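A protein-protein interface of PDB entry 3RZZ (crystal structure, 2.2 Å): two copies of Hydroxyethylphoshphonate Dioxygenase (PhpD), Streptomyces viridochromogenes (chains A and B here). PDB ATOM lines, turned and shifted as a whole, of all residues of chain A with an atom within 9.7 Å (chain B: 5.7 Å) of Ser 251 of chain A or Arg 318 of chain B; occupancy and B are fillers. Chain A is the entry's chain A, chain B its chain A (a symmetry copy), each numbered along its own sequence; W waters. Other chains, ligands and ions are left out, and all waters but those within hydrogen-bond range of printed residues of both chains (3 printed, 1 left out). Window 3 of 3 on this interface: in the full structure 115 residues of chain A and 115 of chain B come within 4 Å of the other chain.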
ATOM      1  N   PHE A 241     -31.752   5.050  -1.682  1.00  0.00           N
ATOM      2  CA  PHE A 241     -31.408   6.470  -1.558  1.00  0.00           C
ATOM      3  C   PHE A 241     -30.044   6.723  -2.212  1.00  0.00           C
ATOM      4  O   PHE A 241     -29.874   7.679  -2.970  1.00  0.00           O
ATOM      5  CB  PHE A 241     -31.343   6.894  -0.077  1.00  0.00           C
ATOM      6  CG  PHE A 241     -32.692   7.039   0.595  1.00  0.00           C
ATOM      7  CD1 PHE A 241     -33.850   6.535   0.011  1.00  0.00           C
ATOM      8  CD2 PHE A 241     -32.795   7.665   1.837  1.00  0.00           C
ATOM      9  CE1 PHE A 241     -35.086   6.647   0.648  1.00  0.00           C
ATOM     10  CE2 PHE A 241     -34.029   7.784   2.488  1.00  0.00           C
ATOM     11  CZ  PHE A 241     -35.177   7.274   1.892  1.00  0.00           C
ATOM     12  N   LEU A 242     -29.078   5.857  -1.920  1.00  0.00           N
ATOM     13  CA  LEU A 242     -27.737   6.002  -2.468  1.00  0.00           C
ATOM     14  C   LEU A 242     -27.733   5.831  -3.984  1.00  0.00           C
ATOM     15  O   LEU A 242     -27.188   6.659  -4.708  1.00  0.00           O
ATOM     16  CB  LEU A 242     -26.791   4.982  -1.821  1.00  0.00           C
ATOM     17  CG  LEU A 242     -26.800   4.951  -0.287  1.00  0.00           C
ATOM     18  CD1 LEU A 242     -25.795   3.912   0.192  1.00  0.00           C
ATOM     19  CD2 LEU A 242     -26.481   6.325   0.282  1.00  0.00           C
ATOM     20  N   ALA A 243     -28.340   4.753  -4.464  1.00  0.00           N
ATOM     21  CA  ALA A 243     -28.406   4.513  -5.902  1.00  0.00           C
ATOM     22  C   ALA A 243     -29.066   5.712  -6.581  1.00  0.00           C
ATOM     23  O   ALA A 243     -28.724   6.069  -7.703  1.00  0.00           O
ATOM     24  CB  ALA A 243     -29.200   3.247  -6.185  1.00  0.00           C
ATOM     25  N   ARG A 244     -30.016   6.322  -5.884  1.00  0.00           N
ATOM     26  CA  ARG A 244     -30.737   7.491  -6.379  1.00  0.00           C
ATOM     27  C   ARG A 244     -29.738   8.632  -6.586  1.00  0.00           C
ATOM     28  O   ARG A 244     -29.860   9.422  -7.520  1.00  0.00           O
ATOM     29  CB  ARG A 244     -31.823   7.887  -5.352  1.00  0.00           C
ATOM     30  CG  ARG A 244     -32.656   9.131  -5.677  1.00  0.00           C
ATOM     31  CD  ARG A 244     -33.424   8.979  -6.977  1.00  0.00           C
ATOM     32  NE  ARG A 244     -34.439  10.015  -7.153  1.00  0.00           N
ATOM     33  CZ  ARG A 244     -35.047  10.267  -8.312  1.00  0.00           C
ATOM     34  NH1 ARG A 244     -34.736   9.562  -9.391  1.00  0.00           N
ATOM     35  NH2 ARG A 244     -35.971  11.216  -8.394  1.00  0.00           N
ATOM     36  N   ARG A 245     -28.731   8.692  -5.719  1.00  0.00           N
ATOM     37  CA  ARG A 245     -27.716   9.738  -5.790  1.00  0.00           C
ATOM     38  C   ARG A 245     -26.377   9.320  -6.405  1.00  0.00           C
ATOM     39  O   ARG A 245     -25.373  10.042  -6.286  1.00  0.00           O
ATOM     40  CB  ARG A 245     -27.488  10.295  -4.389  1.00  0.00           C
ATOM     41  CG  ARG A 245     -28.736  10.911  -3.804  1.00  0.00           C
ATOM     42  CD  ARG A 245     -28.535  11.340  -2.374  1.00  0.00           C
ATOM     43  NE  ARG A 245     -29.733  11.974  -1.832  1.00  0.00           N
ATOM     44  CZ  ARG A 245     -30.906  11.369  -1.687  1.00  0.00           C
ATOM     45  NH1 ARG A 245     -31.058  10.096  -2.047  1.00  0.00           N
ATOM     46  NH2 ARG A 245     -31.926  12.039  -1.171  1.00  0.00           N
ATOM     47  N   ALA A 246     -26.362   8.166  -7.065  1.00  0.00           N
ATOM     48  CA  ALA A 246     -25.147   7.664  -7.704  1.00  0.00           C
ATOM     49  C   ALA A 246     -24.024   7.482  -6.685  1.00  0.00           C
ATOM     50  O   ALA A 246     -22.878   7.844  -6.931  1.00  0.00           O
ATOM     51  CB  ALA A 246     -24.703   8.618  -8.811  1.00  0.00           C
ATOM     52  N   HIS A 247     -24.376   6.923  -5.536  1.00  0.00           N
ATOM     53  CA  HIS A 247     -23.423   6.663  -4.463  1.00  0.00           C
ATOM     54  C   HIS A 247     -23.477   5.175  -4.102  1.00  0.00           C
ATOM     55  O   HIS A 247     -24.507   4.522  -4.270  1.00  0.00           O
ATOM     56  CB  HIS A 247     -23.788   7.470  -3.210  1.00  0.00           C
ATOM     57  CG  HIS A 247     -23.035   8.756  -3.055  1.00  0.00           C
ATOM     58  ND1 HIS A 247     -23.553   9.978  -3.433  1.00  0.00           N
ATOM     59  CD2 HIS A 247     -21.819   9.014  -2.516  1.00  0.00           C
ATOM     60  CE1 HIS A 247     -22.692  10.934  -3.132  1.00  0.00           C
ATOM     61  NE2 HIS A 247     -21.632  10.376  -2.573  1.00  0.00           N
ATOM     62  N   THR A 248     -22.363   4.638  -3.621  1.00  0.00           N
ATOM     63  CA  THR A 248     -22.330   3.245  -3.186  1.00  0.00           C
ATOM     64  C   THR A 248     -22.212   3.383  -1.678  1.00  0.00           C
ATOM     65  O   THR A 248     -22.089   4.500  -1.175  1.00  0.00           O
ATOM     66  CB  THR A 248     -21.087   2.492  -3.716  1.00  0.00           C
ATOM     67  OG1 THR A 248     -19.897   3.168  -3.278  1.00  0.00           O
ATOM     68  CG2 THR A 248     -21.112   2.413  -5.244  1.00  0.00           C
ATOM     69  N   ARG A 249     -22.262   2.282  -0.944  1.00  0.00           N
ATOM     70  CA  ARG A 249     -22.126   2.401   0.505  1.00  0.00           C
ATOM     71  C   ARG A 249     -20.732   2.917   0.864  1.00  0.00           C
ATOM     72  O   ARG A 249     -20.548   3.588   1.880  1.00  0.00           O
ATOM     73  CB  ARG A 249     -22.374   1.056   1.198  1.00  0.00           C
ATOM     74  CG  ARG A 249     -23.824   0.663   1.282  1.00  0.00           C
ATOM     75  CD  ARG A 249     -24.021  -0.527   2.196  1.00  0.00           C
ATOM     76  NE  ARG A 249     -25.413  -0.955   2.201  1.00  0.00           N
ATOM     77  CZ  ARG A 249     -25.942  -1.788   3.088  1.00  0.00           C
ATOM     78  NH1 ARG A 249     -25.196  -2.293   4.063  1.00  0.00           N
ATOM     79  NH2 ARG A 249     -27.222  -2.122   2.994  1.00  0.00           N
ATOM     80  N   THR A 250     -19.758   2.616   0.009  1.00  0.00           N
ATOM     81  CA  THR A 250     -18.379   3.039   0.229  1.00  0.00           C
ATOM     82  C   THR A 250     -18.203   4.536   0.012  1.00  0.00           C
ATOM     83  O   THR A 250     -17.655   5.237   0.869  1.00  0.00           O
ATOM     84  CB  THR A 250     -17.411   2.282  -0.708  1.00  0.00           C
ATOM     85  OG1 THR A 250     -17.512   0.873  -0.464  1.00  0.00           O
ATOM     86  CG2 THR A 250     -15.979   2.735  -0.470  1.00  0.00           C
ATOM     87  N   SER A 251     -18.667   5.026  -1.132  1.00  0.00           N
ATOM     88  CA  SER A 251     -18.546   6.445  -1.438  1.00  0.00           C
ATOM     89  C   SER A 251     -19.341   7.301  -0.458  1.00  0.00           C
ATOM     90  O   SER A 251     -18.890   8.372  -0.047  1.00  0.00           O
ATOM     91  CB  SER A 251     -19.022   6.725  -2.869  1.00  0.00           C
ATOM     92  OG  SER A 251     -20.395   6.401  -3.047  1.00  0.00           O
ATOM     93  N   ALA A 252     -20.524   6.823  -0.088  1.00  0.00           N
ATOM     94  CA  ALA A 252     -21.388   7.548   0.836  1.00  0.00           C
ATOM     95  C   ALA A 252     -20.722   7.684   2.193  1.00  0.00           C
ATOM     96  O   ALA A 252     -20.772   8.749   2.813  1.00  0.00           O
ATOM     97  CB  ALA A 252     -22.719   6.827   0.976  1.00  0.00           C
ATOM     98  N   ALA A 253     -20.094   6.602   2.646  1.00  0.00           N
ATOM     99  CA  ALA A 253     -19.410   6.588   3.936  1.00  0.00           C
ATOM    100  C   ALA A 253     -18.298   7.627   3.972  1.00  0.00           C
ATOM    101  O   ALA A 253     -18.285   8.507   4.832  1.00  0.00           O
ATOM    102  CB  ALA A 253     -18.835   5.206   4.210  1.00  0.00           C
ATOM    103  N   GLU A 254     -17.362   7.518   3.034  1.00  0.00           N
ATOM    104  CA  GLU A 254     -16.249   8.456   2.964  1.00  0.00           C
ATOM    105  C   GLU A 254     -16.787   9.857   2.708  1.00  0.00           C
ATOM    106  O   GLU A 254     -16.128  10.848   3.013  1.00  0.00           O
ATOM    107  CB  GLU A 254     -15.277   8.061   1.849  1.00  0.00           C
ATOM    108  CG  GLU A 254     -14.683   6.669   2.004  1.00  0.00           C
ATOM    109  CD  GLU A 254     -13.604   6.379   0.972  1.00  0.00           C
ATOM    110  OE1 GLU A 254     -13.131   5.219   0.906  1.00  0.00           O
ATOM    111  OE2 GLU A 254     -13.227   7.314   0.230  1.00  0.00           O
ATOM    112  N   ALA A 255     -17.991   9.926   2.147  1.00  0.00           N
ATOM    113  CA  ALA A 255     -18.633  11.202   1.859  1.00  0.00           C
ATOM    114  C   ALA A 255     -19.106  11.840   3.163  1.00  0.00           C
ATOM    115  O   ALA A 255     -19.046  13.057   3.328  1.00  0.00           O
ATOM    116  CB  ALA A 255     -19.814  10.992   0.920  1.00  0.00           C
ATOM    117  N   ALA A 256     -19.577  11.006   4.084  1.00  0.00           N
ATOM    118  CA  ALA A 256     -20.062  11.481   5.370  1.00  0.00           C
ATOM    119  C   ALA A 256     -18.952  11.422   6.416  1.00  0.00           C
ATOM    120  O   ALA A 256     -19.157  11.792   7.574  1.00  0.00           O
ATOM    121  CB  ALA A 256     -21.244  10.639   5.815  1.00  0.00           C
ATOM    122  N   GLY A 257     -17.779  10.957   6.002  1.00  0.00           N
ATOM    123  CA  GLY A 257     -16.646  10.838   6.901  1.00  0.00           C
ATOM    124  C   GLY A 257     -16.886   9.810   7.988  1.00  0.00           C
ATOM    125  O   GLY A 257     -16.463   9.988   9.130  1.00  0.00           O
ATOM    126  N   VAL A 258     -17.570   8.728   7.628  1.00  0.00           N
ATOM    127  CA  VAL A 258     -17.885   7.668   8.577  1.00  0.00           C
ATOM    128  C   VAL A 258     -17.217   6.357   8.179  1.00  0.00           C
ATOM    129  O   VAL A 258     -17.128   6.029   6.997  1.00  0.00           O
ATOM    130  CB  VAL A 258     -19.405   7.443   8.679  1.00  0.00           C
ATOM    131  CG1 VAL A 258     -19.702   6.164   9.443  1.00  0.00           C
ATOM    132  CG2 VAL A 258     -20.074   8.636   9.342  1.00  0.00           C
ATOM    133  N   PRO A 260     -16.817   2.619   7.344  1.00  0.00           N
ATOM    134  CA  PRO A 260     -17.718   1.601   6.798  1.00  0.00           C
ATOM    135  C   PRO A 260     -18.219   0.626   7.862  1.00  0.00           C
ATOM    136  O   PRO A 260     -19.339   0.119   7.773  1.00  0.00           O
ATOM    137  CB  PRO A 260     -16.853   0.918   5.747  1.00  0.00           C
ATOM    138  CG  PRO A 260     -16.043   2.060   5.220  1.00  0.00           C
ATOM    139  CD  PRO A 260     -15.631   2.783   6.485  1.00  0.00           C
ATOM    140  N   LEU A 263     -21.202   2.344   9.709  1.00  0.00           N
ATOM    141  CA  LEU A 263     -22.391   2.458   8.877  1.00  0.00           C
ATOM    142  C   LEU A 263     -23.158   1.141   8.888  1.00  0.00           C
ATOM    143  O   LEU A 263     -24.389   1.133   8.858  1.00  0.00           O
ATOM    144  CB  LEU A 263     -22.016   2.819   7.438  1.00  0.00           C
ATOM    145  CG  LEU A 263     -23.183   2.826   6.440  1.00  0.00           C
ATOM    146  CD1 LEU A 263     -24.321   3.683   6.974  1.00  0.00           C
ATOM    147  CD2 LEU A 263     -22.701   3.351   5.097  1.00  0.00           C
ATOM    148  N   LEU A 282     -24.925  10.849   7.624  1.00  0.00           N
ATOM    149  CA  LEU A 282     -25.155  10.467   6.240  1.00  0.00           C
ATOM    150  C   LEU A 282     -26.196  11.338   5.556  1.00  0.00           C
ATOM    151  O   LEU A 282     -25.988  11.822   4.444  1.00  0.00           O
ATOM    152  CB  LEU A 282     -25.552   8.995   6.131  1.00  0.00           C
ATOM    153  CG  LEU A 282     -24.793   8.152   5.104  1.00  0.00           C
ATOM    154  CD1 LEU A 282     -24.076   9.042   4.103  1.00  0.00           C
ATOM    155  CD2 LEU A 282     -23.813   7.219   5.796  1.00  0.00           C
ATOM    156  N   ALA A 285     -24.949  14.818   4.779  1.00  0.00           N
ATOM    157  CA  ALA A 285     -23.936  14.786   3.730  1.00  0.00           C
ATOM    158  C   ALA A 285     -24.507  14.493   2.343  1.00  0.00           C
ATOM    159  O   ALA A 285     -24.107  15.114   1.359  1.00  0.00           O
ATOM    160  CB  ALA A 285     -22.849  13.777   4.078  1.00  0.00           C
ATOM    161  N   LEU A 286     -25.435  13.545   2.268  1.00  0.00           N
ATOM    162  CA  LEU A 286     -26.011  13.143   0.987  1.00  0.00           C
ATOM    163  C   LEU A 286     -27.298  13.884   0.629  1.00  0.00           C
ATOM    164  O   LEU A 286     -27.789  13.776  -0.493  1.00  0.00           O
ATOM    165  CB  LEU A 286     -26.254  11.631   0.964  1.00  0.00           C
ATOM    166  CG  LEU A 286     -25.007  10.745   0.941  1.00  0.00           C
ATOM    167  CD1 LEU A 286     -24.271  10.887  -0.381  1.00  0.00           C
ATOM    168  CD2 LEU A 286     -24.087  11.076   2.106  1.00  0.00           C
ATOM    169  N   SER B 316     -16.071  14.932  -4.455  1.00  0.00           N
ATOM    170  CA  SER B 316     -17.071  13.867  -4.340  1.00  0.00           C
ATOM    171  C   SER B 316     -17.024  12.808  -5.455  1.00  0.00           C
ATOM    172  O   SER B 316     -17.788  11.838  -5.423  1.00  0.00           O
ATOM    173  CB  SER B 316     -18.472  14.475  -4.322  1.00  0.00           C
ATOM    174  OG  SER B 316     -18.861  14.873  -5.627  1.00  0.00           O
ATOM    175  N   ARG B 317     -16.153  12.987  -6.444  1.00  0.00           N
ATOM    176  CA  ARG B 317     -16.070  12.024  -7.535  1.00  0.00           C
ATOM    177  C   ARG B 317     -15.960  10.594  -7.039  1.00  0.00           C
ATOM    178  O   ARG B 317     -15.228  10.312  -6.095  1.00  0.00           O
ATOM    179  CB  ARG B 317     -14.875  12.327  -8.450  1.00  0.00           C
ATOM    180  CG  ARG B 317     -15.096  13.491  -9.391  1.00  0.00           C
ATOM    181  CD  ARG B 317     -13.881  13.727 -10.256  1.00  0.00           C
ATOM    182  NE  ARG B 317     -12.685  13.920  -9.443  1.00  0.00           N
ATOM    183  CZ  ARG B 317     -11.493  14.242  -9.933  1.00  0.00           C
ATOM    184  NH1 ARG B 317     -10.457  14.396  -9.116  1.00  0.00           N
ATOM    185  NH2 ARG B 317     -11.338  14.418 -11.240  1.00  0.00           N
ATOM    186  N   ARG B 318     -16.711   9.705  -7.682  1.00  0.00           N
ATOM    187  CA  ARG B 318     -16.690   8.291  -7.354  1.00  0.00           C
ATOM    188  C   ARG B 318     -17.195   7.449  -8.517  1.00  0.00           C
ATOM    189  O   ARG B 318     -17.850   7.940  -9.442  1.00  0.00           O
ATOM    190  CB  ARG B 318     -17.528   7.979  -6.096  1.00  0.00           C
ATOM    191  CG  ARG B 318     -19.060   8.129  -6.222  1.00  0.00           C
ATOM    192  CD  ARG B 318     -19.517   9.570  -6.039  1.00  0.00           C
ATOM    193  NE  ARG B 318     -20.968   9.726  -6.134  1.00  0.00           N
ATOM    194  CZ  ARG B 318     -21.593  10.901  -6.117  1.00  0.00           C
ATOM    195  NH1 ARG B 318     -20.902  12.027  -6.009  1.00  0.00           N
ATOM    196  NH2 ARG B 318     -22.916  10.953  -6.209  1.00  0.00           N
ATOM    197  N   THR B 319     -16.862   6.168  -8.470  1.00  0.00           N
ATOM    198  CA  THR B 319     -17.300   5.235  -9.488  1.00  0.00           C
ATOM    199  C   THR B 319     -18.674   4.744  -9.076  1.00  0.00           C
ATOM    200  O   THR B 319     -18.903   4.475  -7.899  1.00  0.00           O
ATOM    201  CB  THR B 319     -16.362   4.036  -9.564  1.00  0.00           C
ATOM    202  OG1 THR B 319     -15.147   4.434 -10.209  1.00  0.00           O
ATOM    203  CG2 THR B 319     -17.015   2.889 -10.329  1.00  0.00           C
ATOM    204  N   PHE B 320     -19.587   4.658 -10.037  1.00  0.00           N
ATOM    205  CA  PHE B 320     -20.936   4.161  -9.783  1.00  0.00           C
ATOM    206  C   PHE B 320     -21.275   3.229 -10.939  1.00  0.00           C
ATOM    207  O   PHE B 320     -21.764   3.662 -11.984  1.00  0.00           O
ATOM    208  CB  PHE B 320     -21.950   5.306  -9.723  1.00  0.00           C
ATOM    209  CG  PHE B 320     -23.363   4.843  -9.483  1.00  0.00           C
ATOM    210  CD1 PHE B 320     -23.701   4.181  -8.303  1.00  0.00           C
ATOM    211  CD2 PHE B 320     -24.350   5.042 -10.446  1.00  0.00           C
ATOM    212  CE1 PHE B 320     -25.001   3.723  -8.089  1.00  0.00           C
ATOM    213  CE2 PHE B 320     -25.650   4.589 -10.242  1.00  0.00           C
ATOM    214  CZ  PHE B 320     -25.976   3.926  -9.060  1.00  0.00           C
ATOM    215  N   TYR B 323     -20.218   4.100 -14.423  1.00  0.00           N
ATOM    216  CA  TYR B 323     -20.185   5.555 -14.480  1.00  0.00           C
ATOM    217  C   TYR B 323     -19.254   6.162 -13.437  1.00  0.00           C
ATOM    218  O   TYR B 323     -18.865   5.514 -12.460  1.00  0.00           O
ATOM    219  CB  TYR B 323     -21.596   6.122 -14.263  1.00  0.00           C
ATOM    220  CG  TYR B 323     -22.637   5.556 -15.203  1.00  0.00           C
ATOM    221  CD1 TYR B 323     -22.594   5.833 -16.573  1.00  0.00           C
ATOM    222  CD2 TYR B 323     -23.655   4.725 -14.729  1.00  0.00           C
ATOM    223  CE1 TYR B 323     -23.541   5.296 -17.447  1.00  0.00           C
ATOM    224  CE2 TYR B 323     -24.600   4.184 -15.589  1.00  0.00           C
ATOM    225  CZ  TYR B 323     -24.542   4.474 -16.947  1.00  0.00           C
ATOM    226  OH  TYR B 323     -25.494   3.957 -17.799  1.00  0.00           O
ATOM    227  N   GLU B 324     -18.888   7.414 -13.681  1.00  0.00           N
ATOM    228  CA  GLU B 324     -18.066   8.193 -12.770  1.00  0.00           C
ATOM    229  C   GLU B 324     -19.048   9.293 -12.356  1.00  0.00           C
ATOM    230  O   GLU B 324     -19.597   9.985 -13.222  1.00  0.00           O
ATOM    231  CB  GLU B 324     -16.857   8.784 -13.508  1.00  0.00           C
ATOM    232  CG  GLU B 324     -16.194   9.965 -12.802  1.00  0.00           C
ATOM    233  CD  GLU B 324     -14.803   9.663 -12.259  1.00  0.00           C
ATOM    234  OE1 GLU B 324     -14.682   8.850 -11.316  1.00  0.00           O
ATOM    235  OE2 GLU B 324     -13.830  10.248 -12.774  1.00  0.00           O
ATOM    236  N   ALA B 325     -19.301   9.445 -11.057  1.00  0.00           N
ATOM    237  CA  ALA B 325     -20.254  10.466 -10.615  1.00  0.00           C
ATOM    238  C   ALA B 325     -19.719  11.484  -9.620  1.00  0.00           C
ATOM    239  O   ALA B 325     -18.826  11.193  -8.821  1.00  0.00           O
ATOM    240  CB  ALA B 325     -21.507   9.807 -10.043  1.00  0.00           C
ATOM    241  N   ALA B 326     -20.274  12.688  -9.700  1.00  0.00           N
ATOM    242  CA  ALA B 326     -19.918  13.782  -8.810  1.00  0.00           C
ATOM    243  C   ALA B 326     -21.239  14.408  -8.365  1.00  0.00           C
ATOM    244  O   ALA B 326     -22.212  14.430  -9.125  1.00  0.00           O
ATOM    245  CB  ALA B 326     -19.058  14.807  -9.533  1.00  0.00           C
ATOM    246  N   SER B 327     -21.269  14.915  -7.138  1.00  0.00           N
ATOM    247  CA  SER B 327     -22.479  15.503  -6.592  1.00  0.00           C
ATOM    248  C   SER B 327     -22.713  16.977  -6.892  1.00  0.00           C
ATOM    249  O   SER B 327     -21.775  17.751  -7.077  1.00  0.00           O
ATOM    250  CB  SER B 327     -22.510  15.310  -5.075  1.00  0.00           C
ATOM    251  OG  SER B 327     -22.586  13.937  -4.731  1.00  0.00           O
ATOM    252  N   SER B 340     -26.815  15.286 -10.059  1.00  0.00           N
ATOM    253  CA  SER B 340     -25.547  14.571 -10.170  1.00  0.00           C
ATOM    254  C   SER B 340     -24.863  14.689 -11.533  1.00  0.00           C
ATOM    255  O   SER B 340     -25.524  14.683 -12.574  1.00  0.00           O
ATOM    256  CB  SER B 340     -25.760  13.085  -9.846  1.00  0.00           C
ATOM    257  OG  SER B 340     -26.171  12.903  -8.498  1.00  0.00           O
HETATM  258  O   HOH W   1     -25.015  13.027  -5.719  1.00  0.00           O
HETATM  259  O   HOH W   2     -17.652   3.664  -5.355  1.00  0.00           O
HETATM  260  O   HOH W   3     -28.375  11.275  -9.551  1.00  0.00           O
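The backbone carbonyl oxygen of Arg 245 of chain A is in hydrogen-bond range of the guanidinium group of Arg 318 of chain B.
The backbone carbonyl oxygen (O) of Ala 246 of chain A is in hydrogen-bond range of the guanidinium group (NE) of Arg 318 of chain B, at 2.8 Å.
A ring nitrogen (ND1) of His 247 of chain A is in hydrogen-bond range of the guanidinium group (NH2) of Arg 318 of chain B.
NH1 of Arg 245 of chain A sits at hydrogen-bond distance from O of Phe 241 of chain A (2.8 Å).
The guanidinium group (NE) of Arg 245 of chain A is in hydrogen-bond range of the backbone carbonyl oxygen (O) of Leu 286 of chain A (3.0 Å).
The backbone carbonyl oxygen of Ser 316 of chain B sits close to the guanidinium group of Arg 318 of chain B, at 3.2 Å.
The backbone NH (N) of Ser 327 of chain B lies within hydrogen-bond range of the side-chain hydroxyl (OG) of Ser 316 of chain B, at 2.8 Å.
N of Ala 325 of chain B is in hydrogen-bond range of O of Arg 318 of chain B (2.6 Å).
NH1 of Arg 318 of chain B is in hydrogen-bond range of OG of Ser 327 of chain B.
Among the printed residues, pairs that only touch across the chains: Ala 243 of chain A with Phe 320 of chain B (3.7 Å), Arg 245 of chain A with Ser 340 of chain B (3.7 Å), Ala 246 of chain A with Phe 320 of chain B (3.7 Å), Ala 246 of chain A with Ala 325 of chain B (3.6 Å), His 247 of chain A with Phe 320 of chain B (3.9 Å), His 247 of chain A with Ser 327 of chain B (3.4 Å) and Ser 251 of chain A with Arg 318 of chain B (3.6 Å).
Ser 251 of chain A touches just one residue of chain B: Arg 318 (3.6 Å).
Gly 257 of chain A touches none of the printed residues of chain B.
Pro 260 of chain A touches none of the printed residues of chain B.
Arg 318 of chain B touches just these residues of chain A: Arg 245, Ala 246, His 247 and Ser 251.
No residue of chain A comes within 4 Å of Thr 319 of chain B.
Of the printed residues of chain A, Phe 320 of chain B touches Ala 243 (3.7 Å), Ala 246 (3.7 Å) and His 247 (3.9 Å).
Ala 325 of chain B touches just one residue of chain A: Ala 246.
No residue of chain A comes within 4 Å of Ala 326 of chain B.
Of the printed residues of chain A, Ser 327 of chain B touches His 247 (3.4 Å).
The nearest residue of chain B that does not touch Ser 251 of chain A is Thr 319 of chain B (5.4 Å).
The nearest printed residue of chain B that does not touch His 247 of chain A is Ser 316 of chain B (5.0 Å).
Of the 11 printed residues of chain B, 5 touch a printed residue of chain A.
Printed residues of chain A that touch a printed residue of chain B: Ala 243, Arg 245, Ala 246, His 247 and Ser 251.
Among the printed residues, no Asp or Glu carboxylate lies within 4 Å of a Lys or Arg side-chain nitrogen of the other chain.
No position is printed for both chains.
Of the 10 pairs that touch across the chains among the printed residues, none has its exchanged pair printed and touching as well.
Water W1 lies within hydrogen-bond range of OG of Ser 327 of chain B (2.8 Å), NH2 of Arg 318 of chain B (3.0 Å), OG of Ser 340 of chain B (3.0 Å) and O of Arg 245 of chain A (3.1 Å).
Water W3 lies within hydrogen-bond range of OG of Ser 340 of chain B and O of Arg 244 of chain A.
Water W2 lies within hydrogen-bond range of O of Thr 319 of chain B (2.9 Å) and OG1 of Thr 248 of chain A (3.1 Å).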
